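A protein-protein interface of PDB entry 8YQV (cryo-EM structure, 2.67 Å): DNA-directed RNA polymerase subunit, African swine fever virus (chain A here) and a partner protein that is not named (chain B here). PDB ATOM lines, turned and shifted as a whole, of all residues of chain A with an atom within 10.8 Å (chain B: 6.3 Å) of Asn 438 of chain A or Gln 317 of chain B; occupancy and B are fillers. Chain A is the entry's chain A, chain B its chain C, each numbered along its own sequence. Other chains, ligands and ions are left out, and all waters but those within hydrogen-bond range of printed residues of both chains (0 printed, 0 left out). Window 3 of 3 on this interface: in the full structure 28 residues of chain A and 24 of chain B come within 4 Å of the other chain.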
ATOM      1  N   ASN A 330     -15.276 -35.167   2.342  1.00  0.00           N
ATOM      2  CA  ASN A 330     -15.536 -35.072   0.911  1.00  0.00           C
ATOM      3  C   ASN A 330     -15.245 -36.441   0.323  1.00  0.00           C
ATOM      4  O   ASN A 330     -14.083 -36.834   0.226  1.00  0.00           O
ATOM      5  CB  ASN A 330     -14.676 -33.994   0.273  1.00  0.00           C
ATOM      6  CG  ASN A 330     -15.084 -33.686  -1.140  1.00  0.00           C
ATOM      7  OD1 ASN A 330     -15.916 -34.364  -1.717  1.00  0.00           O
ATOM      8  ND2 ASN A 330     -14.505 -32.647  -1.703  1.00  0.00           N
ATOM      9  N   ASP A 332     -15.552 -37.500  -2.643  1.00  0.00           N
ATOM     10  CA  ASP A 332     -15.050 -37.465  -4.007  1.00  0.00           C
ATOM     11  C   ASP A 332     -13.558 -37.207  -4.080  1.00  0.00           C
ATOM     12  O   ASP A 332     -13.007 -37.156  -5.181  1.00  0.00           O
ATOM     13  CB  ASP A 332     -15.789 -36.400  -4.803  1.00  0.00           C
ATOM     14  CG  ASP A 332     -17.174 -36.833  -5.191  1.00  0.00           C
ATOM     15  OD1 ASP A 332     -17.337 -37.997  -5.604  1.00  0.00           O
ATOM     16  OD2 ASP A 332     -18.104 -36.018  -5.066  1.00  0.00           O
ATOM     17  N   GLY A 339      -8.673 -31.169  -0.192  1.00  0.00           N
ATOM     18  CA  GLY A 339      -9.330 -30.057  -0.843  1.00  0.00           C
ATOM     19  C   GLY A 339      -8.863 -28.754  -0.237  1.00  0.00           C
ATOM     20  O   GLY A 339      -8.918 -28.571   0.979  1.00  0.00           O
ATOM     21  N   TYR A 340      -8.404 -27.846  -1.092  1.00  0.00           N
ATOM     22  CA  TYR A 340      -7.799 -26.598  -0.650  1.00  0.00           C
ATOM     23  C   TYR A 340      -8.642 -25.430  -1.136  1.00  0.00           C
ATOM     24  O   TYR A 340      -8.869 -25.300  -2.353  1.00  0.00           O
ATOM     25  CB  TYR A 340      -6.362 -26.488  -1.154  1.00  0.00           C
ATOM     26  CG  TYR A 340      -5.490 -25.635  -0.278  1.00  0.00           C
ATOM     27  CD1 TYR A 340      -5.564 -25.739   1.093  1.00  0.00           C
ATOM     28  CD2 TYR A 340      -4.576 -24.751  -0.816  1.00  0.00           C
ATOM     29  CE1 TYR A 340      -4.781 -24.979   1.898  1.00  0.00           C
ATOM     30  CE2 TYR A 340      -3.778 -23.991  -0.007  1.00  0.00           C
ATOM     31  CZ  TYR A 340      -3.888 -24.111   1.351  1.00  0.00           C
ATOM     32  OH  TYR A 340      -3.104 -23.364   2.190  1.00  0.00           O
ATOM     33  N   PRO A 341      -9.128 -24.570  -0.246  1.00  0.00           N
ATOM     34  CA  PRO A 341      -9.904 -23.410  -0.683  1.00  0.00           C
ATOM     35  C   PRO A 341      -9.091 -22.488  -1.577  1.00  0.00           C
ATOM     36  O   PRO A 341      -7.890 -22.302  -1.387  1.00  0.00           O
ATOM     37  CB  PRO A 341     -10.272 -22.721   0.632  1.00  0.00           C
ATOM     38  CG  PRO A 341     -10.117 -23.757   1.656  1.00  0.00           C
ATOM     39  CD  PRO A 341      -9.017 -24.632   1.215  1.00  0.00           C
ATOM     40  N   ILE A 342      -9.768 -21.896  -2.559  1.00  0.00           N
ATOM     41  CA  ILE A 342      -9.067 -21.083  -3.548  1.00  0.00           C
ATOM     42  C   ILE A 342      -8.495 -19.817  -2.924  1.00  0.00           C
ATOM     43  O   ILE A 342      -7.481 -19.300  -3.395  1.00  0.00           O
ATOM     44  CB  ILE A 342      -9.988 -20.759  -4.737  1.00  0.00           C
ATOM     45  CG1 ILE A 342      -9.199 -20.056  -5.840  1.00  0.00           C
ATOM     46  CG2 ILE A 342     -11.169 -19.914  -4.297  1.00  0.00           C
ATOM     47  CD1 ILE A 342      -9.901 -20.009  -7.153  1.00  0.00           C
ATOM     48  N   SER A 343      -9.118 -19.293  -1.870  1.00  0.00           N
ATOM     49  CA  SER A 343      -8.567 -18.121  -1.201  1.00  0.00           C
ATOM     50  C   SER A 343      -7.215 -18.430  -0.579  1.00  0.00           C
ATOM     51  O   SER A 343      -6.319 -17.581  -0.571  1.00  0.00           O
ATOM     52  CB  SER A 343      -9.542 -17.619  -0.146  1.00  0.00           C
ATOM     53  OG  SER A 343      -9.821 -18.631   0.800  1.00  0.00           O
ATOM     54  N   PHE A 344      -7.056 -19.639  -0.042  1.00  0.00           N
ATOM     55  CA  PHE A 344      -5.772 -20.064   0.499  1.00  0.00           C
ATOM     56  C   PHE A 344      -4.747 -20.307  -0.597  1.00  0.00           C
ATOM     57  O   PHE A 344      -3.555 -20.077  -0.384  1.00  0.00           O
ATOM     58  CB  PHE A 344      -5.954 -21.329   1.325  1.00  0.00           C
ATOM     59  CG  PHE A 344      -6.447 -21.082   2.707  1.00  0.00           C
ATOM     60  CD1 PHE A 344      -6.801 -19.820   3.116  1.00  0.00           C
ATOM     61  CD2 PHE A 344      -6.543 -22.115   3.605  1.00  0.00           C
ATOM     62  CE1 PHE A 344      -7.248 -19.604   4.390  1.00  0.00           C
ATOM     63  CE2 PHE A 344      -6.987 -21.899   4.875  1.00  0.00           C
ATOM     64  CZ  PHE A 344      -7.332 -20.648   5.266  1.00  0.00           C
ATOM     65  N   ALA A 345      -5.179 -20.794  -1.759  1.00  0.00           N
ATOM     66  CA  ALA A 345      -4.250 -21.084  -2.842  1.00  0.00           C
ATOM     67  C   ALA A 345      -3.607 -19.830  -3.406  1.00  0.00           C
ATOM     68  O   ALA A 345      -2.515 -19.911  -3.976  1.00  0.00           O
ATOM     69  CB  ALA A 345      -4.963 -21.843  -3.957  1.00  0.00           C
ATOM     70  N   ARG A 346      -4.262 -18.682  -3.279  1.00  0.00           N
ATOM     71  CA  ARG A 346      -3.698 -17.417  -3.714  1.00  0.00           C
ATOM     72  C   ARG A 346      -2.934 -16.703  -2.612  1.00  0.00           C
ATOM     73  O   ARG A 346      -2.303 -15.680  -2.884  1.00  0.00           O
ATOM     74  CB  ARG A 346      -4.808 -16.519  -4.255  1.00  0.00           C
ATOM     75  CG  ARG A 346      -5.858 -17.286  -5.022  1.00  0.00           C
ATOM     76  CD  ARG A 346      -6.402 -16.532  -6.210  1.00  0.00           C
ATOM     77  NE  ARG A 346      -5.356 -16.030  -7.091  1.00  0.00           N
ATOM     78  CZ  ARG A 346      -5.550 -15.112  -8.026  1.00  0.00           C
ATOM     79  NH1 ARG A 346      -6.737 -14.571  -8.228  1.00  0.00           N
ATOM     80  NH2 ARG A 346      -4.525 -14.729  -8.780  1.00  0.00           N
ATOM     81  N   TYR A 373      -7.016 -16.442 -11.694  1.00  0.00           N
ATOM     82  CA  TYR A 373      -6.472 -17.681 -11.156  1.00  0.00           C
ATOM     83  C   TYR A 373      -6.242 -18.695 -12.269  1.00  0.00           C
ATOM     84  O   TYR A 373      -7.072 -18.819 -13.174  1.00  0.00           O
ATOM     85  CB  TYR A 373      -7.416 -18.283 -10.116  1.00  0.00           C
ATOM     86  CG  TYR A 373      -6.849 -19.499  -9.434  1.00  0.00           C
ATOM     87  CD1 TYR A 373      -5.982 -19.374  -8.364  1.00  0.00           C
ATOM     88  CD2 TYR A 373      -7.161 -20.775  -9.875  1.00  0.00           C
ATOM     89  CE1 TYR A 373      -5.452 -20.482  -7.749  1.00  0.00           C
ATOM     90  CE2 TYR A 373      -6.633 -21.883  -9.267  1.00  0.00           C
ATOM     91  CZ  TYR A 373      -5.782 -21.730  -8.206  1.00  0.00           C
ATOM     92  OH  TYR A 373      -5.253 -22.834  -7.597  1.00  0.00           O
ATOM     93  N   THR A 411      -3.916 -27.489  -8.594  1.00  0.00           N
ATOM     94  CA  THR A 411      -4.258 -28.886  -8.374  1.00  0.00           C
ATOM     95  C   THR A 411      -3.101 -29.766  -8.824  1.00  0.00           C
ATOM     96  O   THR A 411      -2.587 -29.613  -9.936  1.00  0.00           O
ATOM     97  CB  THR A 411      -5.538 -29.247  -9.122  1.00  0.00           C
ATOM     98  OG1 THR A 411      -6.641 -28.542  -8.549  1.00  0.00           O
ATOM     99  CG2 THR A 411      -5.816 -30.721  -9.015  1.00  0.00           C
ATOM    100  N   VAL A 434      -6.114 -30.508  -4.186  1.00  0.00           N
ATOM    101  CA  VAL A 434      -7.230 -30.217  -5.076  1.00  0.00           C
ATOM    102  C   VAL A 434      -7.769 -28.856  -4.668  1.00  0.00           C
ATOM    103  O   VAL A 434      -8.210 -28.674  -3.531  1.00  0.00           O
ATOM    104  CB  VAL A 434      -8.321 -31.296  -4.998  1.00  0.00           C
ATOM    105  CG1 VAL A 434      -9.504 -30.912  -5.844  1.00  0.00           C
ATOM    106  CG2 VAL A 434      -7.780 -32.622  -5.445  1.00  0.00           C
ATOM    107  N   VAL A 435      -7.713 -27.894  -5.580  1.00  0.00           N
ATOM    108  CA  VAL A 435      -8.139 -26.538  -5.261  1.00  0.00           C
ATOM    109  C   VAL A 435      -9.647 -26.447  -5.431  1.00  0.00           C
ATOM    110  O   VAL A 435     -10.181 -26.748  -6.502  1.00  0.00           O
ATOM    111  CB  VAL A 435      -7.415 -25.504  -6.131  1.00  0.00           C
ATOM    112  CG1 VAL A 435      -7.973 -24.130  -5.876  1.00  0.00           C
ATOM    113  CG2 VAL A 435      -5.943 -25.520  -5.827  1.00  0.00           C
ATOM    114  N   LEU A 436     -10.335 -26.045  -4.370  1.00  0.00           N
ATOM    115  CA  LEU A 436     -11.782 -25.878  -4.389  1.00  0.00           C
ATOM    116  C   LEU A 436     -12.061 -24.463  -4.865  1.00  0.00           C
ATOM    117  O   LEU A 436     -11.897 -23.502  -4.115  1.00  0.00           O
ATOM    118  CB  LEU A 436     -12.375 -26.131  -3.010  1.00  0.00           C
ATOM    119  CG  LEU A 436     -11.967 -27.417  -2.306  1.00  0.00           C
ATOM    120  CD1 LEU A 436     -12.475 -27.410  -0.890  1.00  0.00           C
ATOM    121  CD2 LEU A 436     -12.484 -28.609  -3.049  1.00  0.00           C
ATOM    122  N   GLU A 437     -12.496 -24.334  -6.108  1.00  0.00           N
ATOM    123  CA  GLU A 437     -12.661 -23.027  -6.723  1.00  0.00           C
ATOM    124  C   GLU A 437     -13.994 -22.374  -6.389  1.00  0.00           C
ATOM    125  O   GLU A 437     -14.249 -21.260  -6.853  1.00  0.00           O
ATOM    126  CB  GLU A 437     -12.469 -23.154  -8.231  1.00  0.00           C
ATOM    127  CG  GLU A 437     -11.002 -23.253  -8.604  1.00  0.00           C
ATOM    128  CD  GLU A 437     -10.768 -23.489 -10.075  1.00  0.00           C
ATOM    129  OE1 GLU A 437     -11.484 -22.893 -10.900  1.00  0.00           O
ATOM    130  OE2 GLU A 437      -9.855 -24.269 -10.407  1.00  0.00           O
ATOM    131  N   ASN A 438     -14.836 -23.026  -5.607  1.00  0.00           N
ATOM    132  CA  ASN A 438     -16.007 -22.377  -5.032  1.00  0.00           C
ATOM    133  C   ASN A 438     -15.555 -21.396  -3.960  1.00  0.00           C
ATOM    134  O   ASN A 438     -14.906 -21.813  -2.992  1.00  0.00           O
ATOM    135  CB  ASN A 438     -16.937 -23.418  -4.432  1.00  0.00           C
ATOM    136  CG  ASN A 438     -18.261 -22.842  -4.002  1.00  0.00           C
ATOM    137  OD1 ASN A 438     -18.592 -21.708  -4.323  1.00  0.00           O
ATOM    138  ND2 ASN A 438     -19.023 -23.620  -3.251  1.00  0.00           N
ATOM    139  N   PRO A 439     -15.864 -20.103  -4.079  1.00  0.00           N
ATOM    140  CA  PRO A 439     -15.368 -19.127  -3.106  1.00  0.00           C
ATOM    141  C   PRO A 439     -16.047 -19.182  -1.751  1.00  0.00           C
ATOM    142  O   PRO A 439     -15.579 -18.521  -0.820  1.00  0.00           O
ATOM    143  CB  PRO A 439     -15.647 -17.791  -3.801  1.00  0.00           C
ATOM    144  CG  PRO A 439     -16.780 -18.065  -4.685  1.00  0.00           C
ATOM    145  CD  PRO A 439     -16.595 -19.458  -5.178  1.00  0.00           C
ATOM    146  N   LYS A 440     -17.123 -19.946  -1.606  1.00  0.00           N
ATOM    147  CA  LYS A 440     -17.886 -19.988  -0.372  1.00  0.00           C
ATOM    148  C   LYS A 440     -17.441 -21.105   0.557  1.00  0.00           C
ATOM    149  O   LYS A 440     -18.056 -21.305   1.607  1.00  0.00           O
ATOM    150  CB  LYS A 440     -19.375 -20.128  -0.685  1.00  0.00           C
ATOM    151  CG  LYS A 440     -20.045 -18.829  -1.095  1.00  0.00           C
ATOM    152  CD  LYS A 440     -21.562 -18.960  -1.123  1.00  0.00           C
ATOM    153  CE  LYS A 440     -22.006 -20.342  -1.589  1.00  0.00           C
ATOM    154  NZ  LYS A 440     -23.290 -20.306  -2.344  1.00  0.00           N
ATOM    155  N   ILE A 441     -16.389 -21.830   0.201  1.00  0.00           N
ATOM    156  CA  ILE A 441     -15.895 -22.955   0.984  1.00  0.00           C
ATOM    157  C   ILE A 441     -14.578 -22.540   1.617  1.00  0.00           C
ATOM    158  O   ILE A 441     -13.645 -22.131   0.918  1.00  0.00           O
ATOM    159  CB  ILE A 441     -15.727 -24.214   0.123  1.00  0.00           C
ATOM    160  CG1 ILE A 441     -17.082 -24.691  -0.380  1.00  0.00           C
ATOM    161  CG2 ILE A 441     -15.059 -25.308   0.909  1.00  0.00           C
ATOM    162  CD1 ILE A 441     -16.982 -25.678  -1.495  1.00  0.00           C
ATOM    163  N   SER A 442     -14.505 -22.638   2.939  1.00  0.00           N
ATOM    164  CA  SER A 442     -13.329 -22.240   3.691  1.00  0.00           C
ATOM    165  C   SER A 442     -12.682 -23.394   4.431  1.00  0.00           C
ATOM    166  O   SER A 442     -11.738 -23.170   5.192  1.00  0.00           O
ATOM    167  CB  SER A 442     -13.689 -21.140   4.694  1.00  0.00           C
ATOM    168  OG  SER A 442     -14.138 -19.974   4.034  1.00  0.00           O
ATOM    169  N   THR A 443     -13.166 -24.612   4.243  1.00  0.00           N
ATOM    170  CA  THR A 443     -12.716 -25.760   5.007  1.00  0.00           C
ATOM    171  C   THR A 443     -11.694 -26.570   4.226  1.00  0.00           C
ATOM    172  O   THR A 443     -11.652 -26.550   2.996  1.00  0.00           O
ATOM    173  CB  THR A 443     -13.899 -26.654   5.381  1.00  0.00           C
ATOM    174  OG1 THR A 443     -14.726 -26.846   4.234  1.00  0.00           O
ATOM    175  CG2 THR A 443     -14.713 -26.033   6.470  1.00  0.00           C
ATOM    176  N   PHE A 444     -10.860 -27.282   4.969  1.00  0.00           N
ATOM    177  CA  PHE A 444      -9.985 -28.296   4.409  1.00  0.00           C
ATOM    178  C   PHE A 444     -10.800 -29.569   4.259  1.00  0.00           C
ATOM    179  O   PHE A 444     -11.290 -30.111   5.249  1.00  0.00           O
ATOM    180  CB  PHE A 444      -8.780 -28.540   5.314  1.00  0.00           C
ATOM    181  CG  PHE A 444      -7.807 -27.409   5.354  1.00  0.00           C
ATOM    182  CD1 PHE A 444      -7.783 -26.462   4.357  1.00  0.00           C
ATOM    183  CD2 PHE A 444      -6.913 -27.293   6.397  1.00  0.00           C
ATOM    184  CE1 PHE A 444      -6.891 -25.430   4.400  1.00  0.00           C
ATOM    185  CE2 PHE A 444      -6.018 -26.259   6.436  1.00  0.00           C
ATOM    186  CZ  PHE A 444      -6.008 -25.329   5.439  1.00  0.00           C
ATOM    187  N   GLN A 445     -10.961 -30.037   3.036  1.00  0.00           N
ATOM    188  CA  GLN A 445     -11.768 -31.215   2.779  1.00  0.00           C
ATOM    189  C   GLN A 445     -10.872 -32.405   2.484  1.00  0.00           C
ATOM    190  O   GLN A 445      -9.866 -32.282   1.785  1.00  0.00           O
ATOM    191  CB  GLN A 445     -12.734 -30.961   1.629  1.00  0.00           C
ATOM    192  CG  GLN A 445     -13.758 -29.914   1.975  1.00  0.00           C
ATOM    193  CD  GLN A 445     -14.696 -29.614   0.850  1.00  0.00           C
ATOM    194  OE1 GLN A 445     -14.581 -30.170  -0.235  1.00  0.00           O
ATOM    195  NE2 GLN A 445     -15.639 -28.725   1.098  1.00  0.00           N
ATOM    196  N   ILE B 283     -18.820 -30.269 -19.655  1.00  0.00           N
ATOM    197  CA  ILE B 283     -19.586 -29.034 -19.759  1.00  0.00           C
ATOM    198  C   ILE B 283     -19.582 -28.350 -18.405  1.00  0.00           C
ATOM    199  O   ILE B 283     -19.942 -28.963 -17.396  1.00  0.00           O
ATOM    200  CB  ILE B 283     -21.027 -29.284 -20.231  1.00  0.00           C
ATOM    201  CG1 ILE B 283     -21.049 -30.285 -21.376  1.00  0.00           C
ATOM    202  CG2 ILE B 283     -21.646 -27.990 -20.691  1.00  0.00           C
ATOM    203  CD1 ILE B 283     -20.417 -29.764 -22.618  1.00  0.00           C
ATOM    204  N   LYS B 284     -19.190 -27.082 -18.382  1.00  0.00           N
ATOM    205  CA  LYS B 284     -19.076 -26.353 -17.130  1.00  0.00           C
ATOM    206  C   LYS B 284     -20.441 -25.884 -16.652  1.00  0.00           C
ATOM    207  O   LYS B 284     -21.286 -25.469 -17.449  1.00  0.00           O
ATOM    208  CB  LYS B 284     -18.143 -25.157 -17.289  1.00  0.00           C
ATOM    209  CG  LYS B 284     -16.707 -25.440 -16.918  1.00  0.00           C
ATOM    210  CD  LYS B 284     -16.433 -25.078 -15.471  1.00  0.00           C
ATOM    211  CE  LYS B 284     -15.412 -26.021 -14.847  1.00  0.00           C
ATOM    212  NZ  LYS B 284     -15.226 -25.763 -13.394  1.00  0.00           N
ATOM    213  N   ASP B 285     -20.647 -25.957 -15.337  1.00  0.00           N
ATOM    214  CA  ASP B 285     -21.875 -25.507 -14.682  1.00  0.00           C
ATOM    215  C   ASP B 285     -23.104 -26.239 -15.202  1.00  0.00           C
ATOM    216  O   ASP B 285     -24.198 -25.676 -15.247  1.00  0.00           O
ATOM    217  CB  ASP B 285     -22.064 -23.996 -14.817  1.00  0.00           C
ATOM    218  CG  ASP B 285     -22.555 -23.356 -13.534  1.00  0.00           C
ATOM    219  OD1 ASP B 285     -22.479 -24.013 -12.475  1.00  0.00           O
ATOM    220  OD2 ASP B 285     -23.017 -22.196 -13.582  1.00  0.00           O
ATOM    221  N   GLU B 286     -22.942 -27.493 -15.598  1.00  0.00           N
ATOM    222  CA  GLU B 286     -24.091 -28.328 -15.888  1.00  0.00           C
ATOM    223  C   GLU B 286     -24.496 -29.112 -14.650  1.00  0.00           C
ATOM    224  O   GLU B 286     -23.774 -29.180 -13.654  1.00  0.00           O
ATOM    225  CB  GLU B 286     -23.811 -29.280 -17.042  1.00  0.00           C
ATOM    226  CG  GLU B 286     -24.156 -28.720 -18.390  1.00  0.00           C
ATOM    227  CD  GLU B 286     -25.629 -28.441 -18.549  1.00  0.00           C
ATOM    228  OE1 GLU B 286     -26.438 -29.070 -17.842  1.00  0.00           O
ATOM    229  OE2 GLU B 286     -25.980 -27.590 -19.389  1.00  0.00           O
ATOM    230  N   VAL B 313     -19.511 -33.831  -9.976  1.00  0.00           N
ATOM    231  CA  VAL B 313     -18.893 -33.716  -8.653  1.00  0.00           C
ATOM    232  C   VAL B 313     -19.239 -32.351  -8.069  1.00  0.00           C
ATOM    233  O   VAL B 313     -19.085 -31.332  -8.759  1.00  0.00           O
ATOM    234  CB  VAL B 313     -17.382 -33.905  -8.753  1.00  0.00           C
ATOM    235  CG1 VAL B 313     -16.728 -33.675  -7.421  1.00  0.00           C
ATOM    236  CG2 VAL B 313     -17.068 -35.284  -9.251  1.00  0.00           C
ATOM    237  N   PRO B 314     -19.729 -32.279  -6.831  1.00  0.00           N
ATOM    238  CA  PRO B 314     -20.146 -30.982  -6.288  1.00  0.00           C
ATOM    239  C   PRO B 314     -19.050 -29.932  -6.257  1.00  0.00           C
ATOM    240  O   PRO B 314     -19.347 -28.750  -6.457  1.00  0.00           O
ATOM    241  CB  PRO B 314     -20.625 -31.343  -4.878  1.00  0.00           C
ATOM    242  CG  PRO B 314     -21.045 -32.743  -4.980  1.00  0.00           C
ATOM    243  CD  PRO B 314     -20.110 -33.390  -5.946  1.00  0.00           C
ATOM    244  N   HIS B 315     -17.797 -30.312  -6.024  1.00  0.00           N
ATOM    245  CA  HIS B 315     -16.731 -29.333  -5.870  1.00  0.00           C
ATOM    246  C   HIS B 315     -16.051 -28.981  -7.183  1.00  0.00           C
ATOM    247  O   HIS B 315     -15.033 -28.284  -7.167  1.00  0.00           O
ATOM    248  CB  HIS B 315     -15.691 -29.816  -4.848  1.00  0.00           C
ATOM    249  CG  HIS B 315     -14.840 -30.958  -5.313  1.00  0.00           C
ATOM    250  ND1 HIS B 315     -13.808 -30.800  -6.210  1.00  0.00           N
ATOM    251  CD2 HIS B 315     -14.840 -32.265  -4.969  1.00  0.00           C
ATOM    252  CE1 HIS B 315     -13.229 -31.967  -6.423  1.00  0.00           C
ATOM    253  NE2 HIS B 315     -13.836 -32.872  -5.681  1.00  0.00           N
ATOM    254  N   LYS B 316     -16.590 -29.425  -8.317  1.00  0.00           N
ATOM    255  CA  LYS B 316     -15.988 -29.138  -9.607  1.00  0.00           C
ATOM    256  C   LYS B 316     -16.857 -28.315 -10.538  1.00  0.00           C
ATOM    257  O   LYS B 316     -16.343 -27.832 -11.550  1.00  0.00           O
ATOM    258  CB  LYS B 316     -15.600 -30.437 -10.320  1.00  0.00           C
ATOM    259  CG  LYS B 316     -14.553 -31.217  -9.580  1.00  0.00           C
ATOM    260  CD  LYS B 316     -13.895 -32.235 -10.465  1.00  0.00           C
ATOM    261  CE  LYS B 316     -12.907 -31.553 -11.383  1.00  0.00           C
ATOM    262  NZ  LYS B 316     -11.877 -30.815 -10.610  1.00  0.00           N
ATOM    263  N   GLN B 317     -18.142 -28.143 -10.236  1.00  0.00           N
ATOM    264  CA  GLN B 317     -19.037 -27.280 -11.008  1.00  0.00           C
ATOM    265  C   GLN B 317     -19.054 -27.639 -12.491  1.00  0.00           C
ATOM    266  O   GLN B 317     -19.054 -26.764 -13.356  1.00  0.00           O
ATOM    267  CB  GLN B 317     -18.678 -25.804 -10.823  1.00  0.00           C
ATOM    268  CG  GLN B 317     -19.144 -25.199  -9.509  1.00  0.00           C
ATOM    269  CD  GLN B 317     -18.019 -24.991  -8.520  1.00  0.00           C
ATOM    270  OE1 GLN B 317     -16.858 -24.851  -8.899  1.00  0.00           O
ATOM    271  NE2 GLN B 317     -18.357 -24.970  -7.241  1.00  0.00           N
ATOM    272  N   GLU B 318     -19.082 -28.933 -12.794  1.00  0.00           N
ATOM    273  CA  GLU B 318     -19.111 -29.370 -14.181  1.00  0.00           C
ATOM    274  C   GLU B 318     -19.727 -30.755 -14.270  1.00  0.00           C
ATOM    275  O   GLU B 318     -19.763 -31.506 -13.294  1.00  0.00           O
ATOM    276  CB  GLU B 318     -17.714 -29.386 -14.794  1.00  0.00           C
ATOM    277  CG  GLU B 318     -16.838 -30.484 -14.252  1.00  0.00           C
ATOM    278  CD  GLU B 318     -15.429 -30.394 -14.764  1.00  0.00           C
ATOM    279  OE1 GLU B 318     -15.133 -29.435 -15.503  1.00  0.00           O
ATOM    280  OE2 GLU B 318     -14.616 -31.277 -14.430  1.00  0.00           O
ATOM    281  N   MET B 319     -20.204 -31.084 -15.465  1.00  0.00           N
ATOM    282  CA  MET B 319     -20.701 -32.410 -15.795  1.00  0.00           C
ATOM    283  C   MET B 319     -19.750 -33.043 -16.796  1.00  0.00           C
ATOM    284  O   MET B 319     -19.472 -32.456 -17.843  1.00  0.00           O
ATOM    285  CB  MET B 319     -22.112 -32.337 -16.378  1.00  0.00           C
ATOM    286  CG  MET B 319     -22.741 -33.673 -16.704  1.00  0.00           C
ATOM    287  SD  MET B 319     -22.490 -34.227 -18.398  1.00  0.00           S
ATOM    288  CE  MET B 319     -23.105 -32.835 -19.323  1.00  0.00           C
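Of the printed residues of chain B, Asp 332 of chain A touches Val 313 and Pro 314. Of the printed residues of chain B, Leu 436 of chain A touches His 315. Printed residues of chain B within 4 Å of Asn 438 of chain A: Gln 317 (3.5 Å). Lys 440 of chain A touches none of the printed residues of chain B. No residue of chain A comes within 4 Å of Lys 284 of chain B. No residue of chain A comes within 4 Å of Asp 285 of chain B. Printed residues of chain A within 4 Å of Val 313 of chain B: Asp 332. Printed residues of chain A within 4 Å of Pro 314 of chain B: Asp 332 (3.4 Å). Printed residues of chain A within 4 Å of His 315 of chain B: Asn 330, Val 434 and Leu 436. The nearest residue of chain B that does not touch Asn 438 of chain A is His 315 of chain B (5.5 Å). The nearest printed residue of chain A that does not touch Val 313 of chain B is Asn 330 of chain A (5.8 Å).
The backbone NH of Asp 332 of chain A lies close to the side-chain amide oxygen of Asn 330 of chain A (3.3 Å). ND2 of Asn 330 of chain A sits at hydrogen-bond distance from OE1 of Gln 445 of chain A (2.9 Å). O of Val 434 of chain A is in hydrogen-bond range of N of Tyr 340 of chain A. The backbone carbonyl oxygen (O) of Tyr 340 of chain A lies within hydrogen-bond range of the backbone NH (N) of Leu 436 of chain A, 2.6 Å away. The backbone carbonyl oxygen (O) of Leu 436 of chain A sits at hydrogen-bond distance from the backbone NH (N) of Ile 342 of chain A. The backbone NH of Asp 285 of chain B lies within hydrogen-bond range of the backbone carbonyl oxygen of Gln 317 of chain B (2.7 Å).
Among the printed residues, pairs that only touch across the chains: Asn 330 of chain A with His 315 of chain B (3.3 Å), Asp 332 of chain A with Val 313 of chain B (3.6 Å), Asp 332 of chain A with Pro 314 of chain B (3.4 Å), Val 434 of chain A with His 315 of chain B (3.9 Å), Leu 436 of chain A with His 315 of chain B (3.9 Å) and Asn 438 of chain A with Gln 317 of chain B (3.5 Å).
Hydrophobic or aromatic side chains of chain B within 4 Å of the printed part of chain A: Val 313, Pro 314 and His 315. Among the printed residues, no Asp or Glu carboxylate lies within 4 Å of a Lys or Arg side-chain nitrogen of the other chain.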
